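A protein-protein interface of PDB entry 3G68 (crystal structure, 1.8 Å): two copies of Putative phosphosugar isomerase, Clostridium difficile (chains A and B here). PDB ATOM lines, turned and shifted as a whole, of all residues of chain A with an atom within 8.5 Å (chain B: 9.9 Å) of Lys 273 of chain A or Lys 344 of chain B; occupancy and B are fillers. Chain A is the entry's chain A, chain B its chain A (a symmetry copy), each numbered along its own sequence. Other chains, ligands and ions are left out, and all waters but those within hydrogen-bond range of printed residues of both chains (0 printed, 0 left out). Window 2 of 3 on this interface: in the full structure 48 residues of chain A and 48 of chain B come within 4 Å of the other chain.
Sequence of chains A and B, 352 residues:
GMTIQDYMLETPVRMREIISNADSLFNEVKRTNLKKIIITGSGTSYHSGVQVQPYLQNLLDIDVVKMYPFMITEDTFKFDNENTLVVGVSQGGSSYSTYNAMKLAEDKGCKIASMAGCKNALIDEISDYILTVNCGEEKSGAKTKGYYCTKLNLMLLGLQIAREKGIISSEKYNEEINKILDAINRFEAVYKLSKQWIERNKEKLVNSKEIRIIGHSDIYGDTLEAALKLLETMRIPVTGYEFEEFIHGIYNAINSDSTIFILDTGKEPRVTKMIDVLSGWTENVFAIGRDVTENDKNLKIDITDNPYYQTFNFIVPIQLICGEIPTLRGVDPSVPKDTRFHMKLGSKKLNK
CE1 of His 342 of chain B touches O of Ile 247 of chain A (3.2 Å). Arg 270 of chain A touches Leu 345 of chain B. Lys 273 of chain A touches Lys 344 of chain B (CG to O, 3.95 Å). Leu 345 of chain B touches Met 274 of chain A. Val 277 of chain A touches Phe 341 of chain B. Lys 344 of chain B touches Val 277 of chain A (CB to CG2, 3.99 Å). Trp 281 of chain A touches Lys 337 of chain B (CE2 to CE, 3.5 Å). Trp 281 of chain A touches Asp 338 of chain B (CZ2 to OD2, 3.6 Å). Trp 281 of chain A touches Phe 341 of chain B (CH2 to CD1, 3.8 Å).
No position is printed for both chains. Of the 9 pairs that touch across the chains among the printed residues, none has its exchanged pair printed and touching as well.
Printed residues of chain A that touch a printed residue of chain B: Ile 247, Arg 270, Lys 273, Met 274, Val 277 and Trp 281. Hydrophobic or aromatic side chains of chain A that line the printed part of chain B: Ile 247, Met 274, Val 277 and Trp 281. Of the 9 printed residues of chain B, 6 touch a printed residue of chain A. Hydrophobic or aromatic side chains of chain B that line the printed part of chain A: Phe 341, His 342 and Leu 345. Among the printed residues, no Asp or Glu carboxylate lies within 4 Å of a Lys or Arg side-chain nitrogen of the other chain.
Phe 243 of chain A touches none of the printed residues of chain B. Of the printed residues of chain B, Ile 247 of chain A touches His 342 (3.2 Å). Of the printed residues of chain B, Arg 270 of chain A touches Leu 345. No residue of chain B comes within 4 Å of Thr 272 of chain A. No residue of chain B comes within 4 Å of Asp 276 of chain A. Leu 278 of chain A touches none of the printed residues of chain B. Of the printed residues of chain B, Trp 281 of chain A touches Lys 337 (3.5 Å), Asp 338 (3.6 Å) and Phe 341 (3.8 Å). Of the printed residues of chain A, Lys 337 of chain B touches Trp 281. No residue of chain A comes within 4 Å of Met 343 of chain B. Of the printed residues of chain A, Lys 344 of chain B touches Lys 273 and Val 277. The nearest printed residue of chain A that does not touch Lys 337 of chain B is Val 277 of chain A (7.3 Å).
The side-chain carboxylate of Glu 268 of chain A is in salt-bridge range of the guanidinium group of Arg 270 of chain A (2.9 Å). The side-chain carboxylate of Asp 338 of chain B sits at hydrogen-bond distance from the backbone NH of Arg 340 of chain B, 2.8 Å away. OD1 of Asp 338 of chain B sits at hydrogen-bond distance from N of Phe 341 of chain B. OD2 of Asp 338 of chain B is in salt-bridge range of NZ of Lys 344 of chain B (2.7 Å).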
ATOM      1  N   PHE A 243      -5.360  35.384  12.759  1.00  0.00           N
ATOM      2  CA  PHE A 243      -5.538  34.205  11.902  1.00  0.00           C
ATOM      3  C   PHE A 243      -5.141  32.872  12.546  1.00  0.00           C
ATOM      4  O   PHE A 243      -5.906  31.910  12.546  1.00  0.00           O
ATOM      5  CB  PHE A 243      -4.735  34.430  10.594  1.00  0.00           C
ATOM      6  CG  PHE A 243      -5.008  33.429   9.530  1.00  0.00           C
ATOM      7  CD1 PHE A 243      -4.327  32.221   9.509  1.00  0.00           C
ATOM      8  CD2 PHE A 243      -5.913  33.715   8.506  1.00  0.00           C
ATOM      9  CE1 PHE A 243      -4.556  31.309   8.523  1.00  0.00           C
ATOM     10  CE2 PHE A 243      -6.156  32.784   7.493  1.00  0.00           C
ATOM     11  CZ  PHE A 243      -5.478  31.582   7.502  1.00  0.00           C
ATOM     12  N   ILE A 247      -7.517  29.493  14.146  1.00  0.00           N
ATOM     13  CA  ILE A 247      -7.329  28.077  13.855  1.00  0.00           C
ATOM     14  C   ILE A 247      -7.414  27.205  15.109  1.00  0.00           C
ATOM     15  O   ILE A 247      -7.859  26.052  15.037  1.00  0.00           O
ATOM     16  CB  ILE A 247      -5.993  27.852  13.068  1.00  0.00           C
ATOM     17  CG1 ILE A 247      -6.101  28.542  11.703  1.00  0.00           C
ATOM     18  CG2 ILE A 247      -5.655  26.330  12.974  1.00  0.00           C
ATOM     19  CD1 ILE A 247      -4.770  28.630  10.940  1.00  0.00           C
ATOM     20  N   ILE A 262     -12.577  38.738   6.354  1.00  0.00           N
ATOM     21  CA  ILE A 262     -11.152  38.373   6.338  1.00  0.00           C
ATOM     22  C   ILE A 262     -10.354  39.580   5.849  1.00  0.00           C
ATOM     23  O   ILE A 262     -10.579  40.084   4.714  1.00  0.00           O
ATOM     24  CB  ILE A 262     -10.899  37.141   5.462  1.00  0.00           C
ATOM     25  CG1 ILE A 262     -11.610  35.928   6.113  1.00  0.00           C
ATOM     26  CG2 ILE A 262      -9.362  36.851   5.341  1.00  0.00           C
ATOM     27  CD1 ILE A 262     -11.678  34.743   5.204  1.00  0.00           C
ATOM     28  N   GLU A 268      -0.145  35.895   4.459  1.00  0.00           N
ATOM     29  CA  GLU A 268      -0.595  34.586   4.884  1.00  0.00           C
ATOM     30  C   GLU A 268      -1.003  33.722   3.680  1.00  0.00           C
ATOM     31  O   GLU A 268      -2.088  33.909   3.130  1.00  0.00           O
ATOM     32  CB  GLU A 268      -1.775  34.746   5.850  1.00  0.00           C
ATOM     33  CG  GLU A 268      -2.382  33.417   6.326  1.00  0.00           C
ATOM     34  CD  GLU A 268      -1.347  32.524   6.965  1.00  0.00           C
ATOM     35  OE1 GLU A 268      -0.946  32.845   8.100  1.00  0.00           O
ATOM     36  OE2 GLU A 268      -0.928  31.522   6.322  1.00  0.00           O
ATOM     37  N   PRO A 269      -0.158  32.740   3.299  1.00  0.00           N
ATOM     38  CA  PRO A 269      -0.481  31.897   2.151  1.00  0.00           C
ATOM     39  C   PRO A 269      -1.667  30.961   2.362  1.00  0.00           C
ATOM     40  O   PRO A 269      -2.227  30.460   1.391  1.00  0.00           O
ATOM     41  CB  PRO A 269       0.814  31.103   1.920  1.00  0.00           C
ATOM     42  CG  PRO A 269       1.406  30.994   3.245  1.00  0.00           C
ATOM     43  CD  PRO A 269       1.125  32.331   3.906  1.00  0.00           C
ATOM     44  N   ARG A 270      -2.064  30.729   3.606  1.00  0.00           N
ATOM     45  CA  ARG A 270      -3.223  29.880   3.874  1.00  0.00           C
ATOM     46  C   ARG A 270      -4.576  30.625   3.787  1.00  0.00           C
ATOM     47  O   ARG A 270      -5.595  29.998   4.011  1.00  0.00           O
ATOM     48  CB  ARG A 270      -3.091  29.232   5.245  1.00  0.00           C
ATOM     49  CG  ARG A 270      -1.866  28.341   5.399  1.00  0.00           C
ATOM     50  CD  ARG A 270      -1.754  27.889   6.847  1.00  0.00           C
ATOM     51  NE  ARG A 270      -1.390  29.011   7.708  1.00  0.00           N
ATOM     52  CZ  ARG A 270      -1.314  28.961   9.041  1.00  0.00           C
ATOM     53  NH1 ARG A 270      -1.536  27.843   9.710  1.00  0.00           N
ATOM     54  NH2 ARG A 270      -0.977  30.061   9.705  1.00  0.00           N
ATOM     55  N   VAL A 271      -4.599  31.919   3.452  1.00  0.00           N
ATOM     56  CA  VAL A 271      -5.876  32.656   3.414  1.00  0.00           C
ATOM     57  C   VAL A 271      -6.863  32.035   2.436  1.00  0.00           C
ATOM     58  O   VAL A 271      -8.030  31.862   2.763  1.00  0.00           O
ATOM     59  CB  VAL A 271      -5.699  34.177   3.104  1.00  0.00           C
ATOM     60  CG1 VAL A 271      -7.047  34.854   2.908  1.00  0.00           C
ATOM     61  CG2 VAL A 271      -4.990  34.851   4.251  1.00  0.00           C
ATOM     62  N   THR A 272      -6.389  31.679   1.239  1.00  0.00           N
ATOM     63  CA  THR A 272      -7.259  31.052   0.242  1.00  0.00           C
ATOM     64  C   THR A 272      -7.902  29.773   0.751  1.00  0.00           C
ATOM     65  O   THR A 272      -9.111  29.586   0.590  1.00  0.00           O
ATOM     66  CB  THR A 272      -6.490  30.778  -1.053  1.00  0.00           C
ATOM     67  OG1 THR A 272      -5.972  32.010  -1.553  1.00  0.00           O
ATOM     68  CG2 THR A 272      -7.409  30.164  -2.062  1.00  0.00           C
ATOM     69  N   LYS A 273      -7.114  28.905   1.388  1.00  0.00           N
ATOM     70  CA  LYS A 273      -7.661  27.675   1.989  1.00  0.00           C
ATOM     71  C   LYS A 273      -8.687  28.007   3.053  1.00  0.00           C
ATOM     72  O   LYS A 273      -9.722  27.373   3.111  1.00  0.00           O
ATOM     73  CB  LYS A 273      -6.587  26.746   2.577  1.00  0.00           C
ATOM     74  CG  LYS A 273      -5.794  25.934   1.511  1.00  0.00           C
ATOM     75  N   MET A 274      -8.415  29.014   3.885  1.00  0.00           N
ATOM     76  CA  MET A 274      -9.362  29.425   4.945  1.00  0.00           C
ATOM     77  C   MET A 274     -10.684  29.894   4.344  1.00  0.00           C
ATOM     78  O   MET A 274     -11.743  29.494   4.802  1.00  0.00           O
ATOM     79  CB  MET A 274      -8.765  30.573   5.781  1.00  0.00           C
ATOM     80  CG  MET A 274      -9.678  31.137   6.868  1.00  0.00           C
ATOM     81  SD  MET A 274      -9.939  29.798   8.270  1.00  0.00           S
ATOM     82  CE  MET A 274      -8.242  30.180   9.190  1.00  0.00           C
ATOM     83  N   ILE A 275     -10.608  30.785   3.365  1.00  0.00           N
ATOM     84  CA  ILE A 275     -11.802  31.271   2.641  1.00  0.00           C
ATOM     85  C   ILE A 275     -12.626  30.084   2.093  1.00  0.00           C
ATOM     86  O   ILE A 275     -13.841  30.020   2.297  1.00  0.00           O
ATOM     87  CB  ILE A 275     -11.421  32.294   1.537  1.00  0.00           C
ATOM     88  CG1 ILE A 275     -10.931  33.624   2.160  1.00  0.00           C
ATOM     89  CG2 ILE A 275     -12.621  32.592   0.610  1.00  0.00           C
ATOM     90  CD1 ILE A 275     -10.210  34.563   1.145  1.00  0.00           C
ATOM     91  N   ASP A 276     -11.955  29.101   1.493  1.00  0.00           N
ATOM     92  CA  ASP A 276     -12.627  27.904   0.970  1.00  0.00           C
ATOM     93  C   ASP A 276     -13.348  27.107   2.013  1.00  0.00           C
ATOM     94  O   ASP A 276     -14.521  26.722   1.814  1.00  0.00           O
ATOM     95  CB  ASP A 276     -11.629  26.900   0.381  1.00  0.00           C
ATOM     96  CG  ASP A 276     -11.042  27.325  -0.915  1.00  0.00           C
ATOM     97  OD1 ASP A 276     -11.412  28.389  -1.460  1.00  0.00           O
ATOM     98  OD2 ASP A 276     -10.188  26.537  -1.381  1.00  0.00           O
ATOM     99  N   VAL A 277     -12.648  26.793   3.105  1.00  0.00           N
ATOM    100  CA  VAL A 277     -13.256  25.978   4.151  1.00  0.00           C
ATOM    101  C   VAL A 277     -14.454  26.693   4.790  1.00  0.00           C
ATOM    102  O   VAL A 277     -15.522  26.085   4.997  1.00  0.00           O
ATOM    103  CB  VAL A 277     -12.231  25.489   5.194  1.00  0.00           C
ATOM    104  CG1 VAL A 277     -12.937  24.736   6.315  1.00  0.00           C
ATOM    105  CG2 VAL A 277     -11.217  24.554   4.521  1.00  0.00           C
ATOM    106  N   LEU A 278     -14.291  27.981   5.070  1.00  0.00           N
ATOM    107  CA  LEU A 278     -15.371  28.768   5.657  1.00  0.00           C
ATOM    108  C   LEU A 278     -16.537  28.913   4.689  1.00  0.00           C
ATOM    109  O   LEU A 278     -17.689  28.841   5.112  1.00  0.00           O
ATOM    110  CB  LEU A 278     -14.875  30.159   6.081  1.00  0.00           C
ATOM    111  CG  LEU A 278     -13.832  30.220   7.184  1.00  0.00           C
ATOM    112  CD1 LEU A 278     -13.384  31.683   7.420  1.00  0.00           C
ATOM    113  CD2 LEU A 278     -14.310  29.584   8.479  1.00  0.00           C
ATOM    114  N   SER A 279     -16.238  29.111   3.399  1.00  0.00           N
ATOM    115  CA  SER A 279     -17.264  29.246   2.365  1.00  0.00           C
ATOM    116  C   SER A 279     -18.082  27.986   2.196  1.00  0.00           C
ATOM    117  O   SER A 279     -19.225  28.042   1.731  1.00  0.00           O
ATOM    118  CB  SER A 279     -16.669  29.679   1.040  1.00  0.00           C
ATOM    119  OG  SER A 279     -16.268  31.007   1.163  1.00  0.00           O
ATOM    120  N   GLY A 280     -17.506  26.850   2.592  1.00  0.00           N
ATOM    121  CA  GLY A 280     -18.221  25.615   2.636  1.00  0.00           C
ATOM    122  C   GLY A 280     -19.282  25.587   3.717  1.00  0.00           C
ATOM    123  O   GLY A 280     -20.248  24.820   3.598  1.00  0.00           O
ATOM    124  N   TRP A 281     -19.118  26.403   4.763  1.00  0.00           N
ATOM    125  CA  TRP A 281     -20.069  26.448   5.871  1.00  0.00           C
ATOM    126  C   TRP A 281     -21.032  27.616   5.840  1.00  0.00           C
ATOM    127  O   TRP A 281     -22.134  27.513   6.383  1.00  0.00           O
ATOM    128  CB  TRP A 281     -19.328  26.462   7.207  1.00  0.00           C
ATOM    129  CG  TRP A 281     -18.498  25.238   7.456  1.00  0.00           C
ATOM    130  CD1 TRP A 281     -18.784  23.963   7.084  1.00  0.00           C
ATOM    131  CD2 TRP A 281     -17.296  25.164   8.245  1.00  0.00           C
ATOM    132  NE1 TRP A 281     -17.800  23.105   7.537  1.00  0.00           N
ATOM    133  CE2 TRP A 281     -16.876  23.818   8.243  1.00  0.00           C
ATOM    134  CE3 TRP A 281     -16.528  26.109   8.925  1.00  0.00           C
ATOM    135  CZ2 TRP A 281     -15.723  23.389   8.915  1.00  0.00           C
ATOM    136  CZ3 TRP A 281     -15.374  25.685   9.581  1.00  0.00           C
ATOM    137  CH2 TRP A 281     -14.981  24.334   9.558  1.00  0.00           C
ATOM    138  N   LYS B 337     -16.067  19.925  15.433  1.00  0.00           N
ATOM    139  CA  LYS B 337     -16.955  20.095  14.266  1.00  0.00           C
ATOM    140  C   LYS B 337     -16.421  19.419  13.013  1.00  0.00           C
ATOM    141  O   LYS B 337     -17.176  18.795  12.254  1.00  0.00           O
ATOM    142  CB  LYS B 337     -17.112  21.589  13.970  1.00  0.00           C
ATOM    143  CG  LYS B 337     -17.922  21.949  12.733  1.00  0.00           C
ATOM    144  CD  LYS B 337     -17.872  23.456  12.521  1.00  0.00           C
ATOM    145  CE  LYS B 337     -18.630  23.883  11.263  1.00  0.00           C
ATOM    146  NZ  LYS B 337     -20.097  23.928  11.460  1.00  0.00           N
ATOM    147  N   ASP B 338     -15.122  19.586  12.801  1.00  0.00           N
ATOM    148  CA  ASP B 338     -14.439  19.051  11.646  1.00  0.00           C
ATOM    149  C   ASP B 338     -13.087  18.539  12.140  1.00  0.00           C
ATOM    150  O   ASP B 338     -12.216  19.319  12.531  1.00  0.00           O
ATOM    151  CB  ASP B 338     -14.285  20.152  10.589  1.00  0.00           C
ATOM    152  CG  ASP B 338     -13.683  19.653   9.281  1.00  0.00           C
ATOM    153  OD1 ASP B 338     -13.109  18.534   9.235  1.00  0.00           O
ATOM    154  OD2 ASP B 338     -13.776  20.411   8.287  1.00  0.00           O
ATOM    155  N   THR B 339     -12.946  17.217  12.132  1.00  0.00           N
ATOM    156  CA  THR B 339     -11.715  16.559  12.547  1.00  0.00           C
ATOM    157  C   THR B 339     -10.559  16.822  11.548  1.00  0.00           C
ATOM    158  O   THR B 339      -9.374  16.764  11.928  1.00  0.00           O
ATOM    159  CB  THR B 339     -11.960  15.032  12.717  1.00  0.00           C
ATOM    160  OG1 THR B 339     -12.430  14.476  11.475  1.00  0.00           O
ATOM    161  CG2 THR B 339     -12.995  14.782  13.829  1.00  0.00           C
ATOM    162  N   ARG B 340     -10.918  17.136  10.296  1.00  0.00           N
ATOM    163  CA  ARG B 340      -9.960  17.425   9.223  1.00  0.00           C
ATOM    164  C   ARG B 340      -9.667  18.916   9.002  1.00  0.00           C
ATOM    165  O   ARG B 340      -8.959  19.262   8.051  1.00  0.00           O
ATOM    166  CB  ARG B 340     -10.472  16.828   7.900  1.00  0.00           C
ATOM    167  N   PHE B 341     -10.173  19.793   9.873  1.00  0.00           N
ATOM    168  CA  PHE B 341      -9.985  21.244   9.683  1.00  0.00           C
ATOM    169  C   PHE B 341      -8.525  21.660   9.608  1.00  0.00           C
ATOM    170  O   PHE B 341      -8.137  22.405   8.705  1.00  0.00           O
ATOM    171  CB  PHE B 341     -10.653  22.056  10.801  1.00  0.00           C
ATOM    172  CG  PHE B 341     -10.439  23.537  10.663  1.00  0.00           C
ATOM    173  CD1 PHE B 341     -11.168  24.270   9.727  1.00  0.00           C
ATOM    174  CD2 PHE B 341      -9.486  24.198  11.438  1.00  0.00           C
ATOM    175  CE1 PHE B 341     -10.977  25.655   9.577  1.00  0.00           C
ATOM    176  CE2 PHE B 341      -9.305  25.587  11.310  1.00  0.00           C
ATOM    177  CZ  PHE B 341     -10.050  26.313  10.370  1.00  0.00           C
ATOM    178  N   HIS B 342      -7.739  21.189  10.574  1.00  0.00           N
ATOM    179  CA  HIS B 342      -6.309  21.507  10.641  1.00  0.00           C
ATOM    180  C   HIS B 342      -5.576  20.935   9.415  1.00  0.00           C
ATOM    181  O   HIS B 342      -4.778  21.633   8.779  1.00  0.00           O
ATOM    182  CB  HIS B 342      -5.700  21.028  11.972  1.00  0.00           C
ATOM    183  CG  HIS B 342      -6.285  21.704  13.187  1.00  0.00           C
ATOM    184  ND1 HIS B 342      -5.755  22.857  13.733  1.00  0.00           N
ATOM    185  CD2 HIS B 342      -7.358  21.390  13.953  1.00  0.00           C
ATOM    186  CE1 HIS B 342      -6.473  23.218  14.784  1.00  0.00           C
ATOM    187  NE2 HIS B 342      -7.453  22.346  14.939  1.00  0.00           N
ATOM    188  N   MET B 343      -5.886  19.686   9.065  1.00  0.00           N
ATOM    189  CA  MET B 343      -5.316  19.049   7.867  1.00  0.00           C
ATOM    190  C   MET B 343      -5.663  19.857   6.598  1.00  0.00           C
ATOM    191  O   MET B 343      -4.839  19.962   5.689  1.00  0.00           O
ATOM    192  CB  MET B 343      -5.790  17.594   7.728  1.00  0.00           C
ATOM    193  N   LYS B 344      -6.870  20.431   6.554  1.00  0.00           N
ATOM    194  CA  LYS B 344      -7.313  21.258   5.419  1.00  0.00           C
ATOM    195  C   LYS B 344      -6.561  22.599   5.303  1.00  0.00           C
ATOM    196  O   LYS B 344      -6.317  23.071   4.185  1.00  0.00           O
ATOM    197  CB  LYS B 344      -8.823  21.510   5.489  1.00  0.00           C
ATOM    198  CG  LYS B 344      -9.677  20.291   5.197  1.00  0.00           C
ATOM    199  CD  LYS B 344     -11.096  20.495   5.717  1.00  0.00           C
ATOM    200  CE  LYS B 344     -12.016  19.337   5.349  1.00  0.00           C
ATOM    201  NZ  LYS B 344     -13.419  19.607   5.766  1.00  0.00           N
ATOM    202  N   LEU B 345      -6.206  23.202   6.439  1.00  0.00           N
ATOM    203  CA  LEU B 345      -5.468  24.474   6.445  1.00  0.00           C
ATOM    204  C   LEU B 345      -3.984  24.259   6.143  1.00  0.00           C
ATOM    205  O   LEU B 345      -3.387  25.032   5.383  1.00  0.00           O
ATOM    206  CB  LEU B 345      -5.660  25.241   7.768  1.00  0.00           C
ATOM    207  CG  LEU B 345      -6.849  26.212   7.827  1.00  0.00           C
ATOM    208  CD1 LEU B 345      -6.504  27.493   7.094  1.00  0.00           C
ATOM    209  CD2 LEU B 345      -8.139  25.617   7.271  1.00  0.00           C
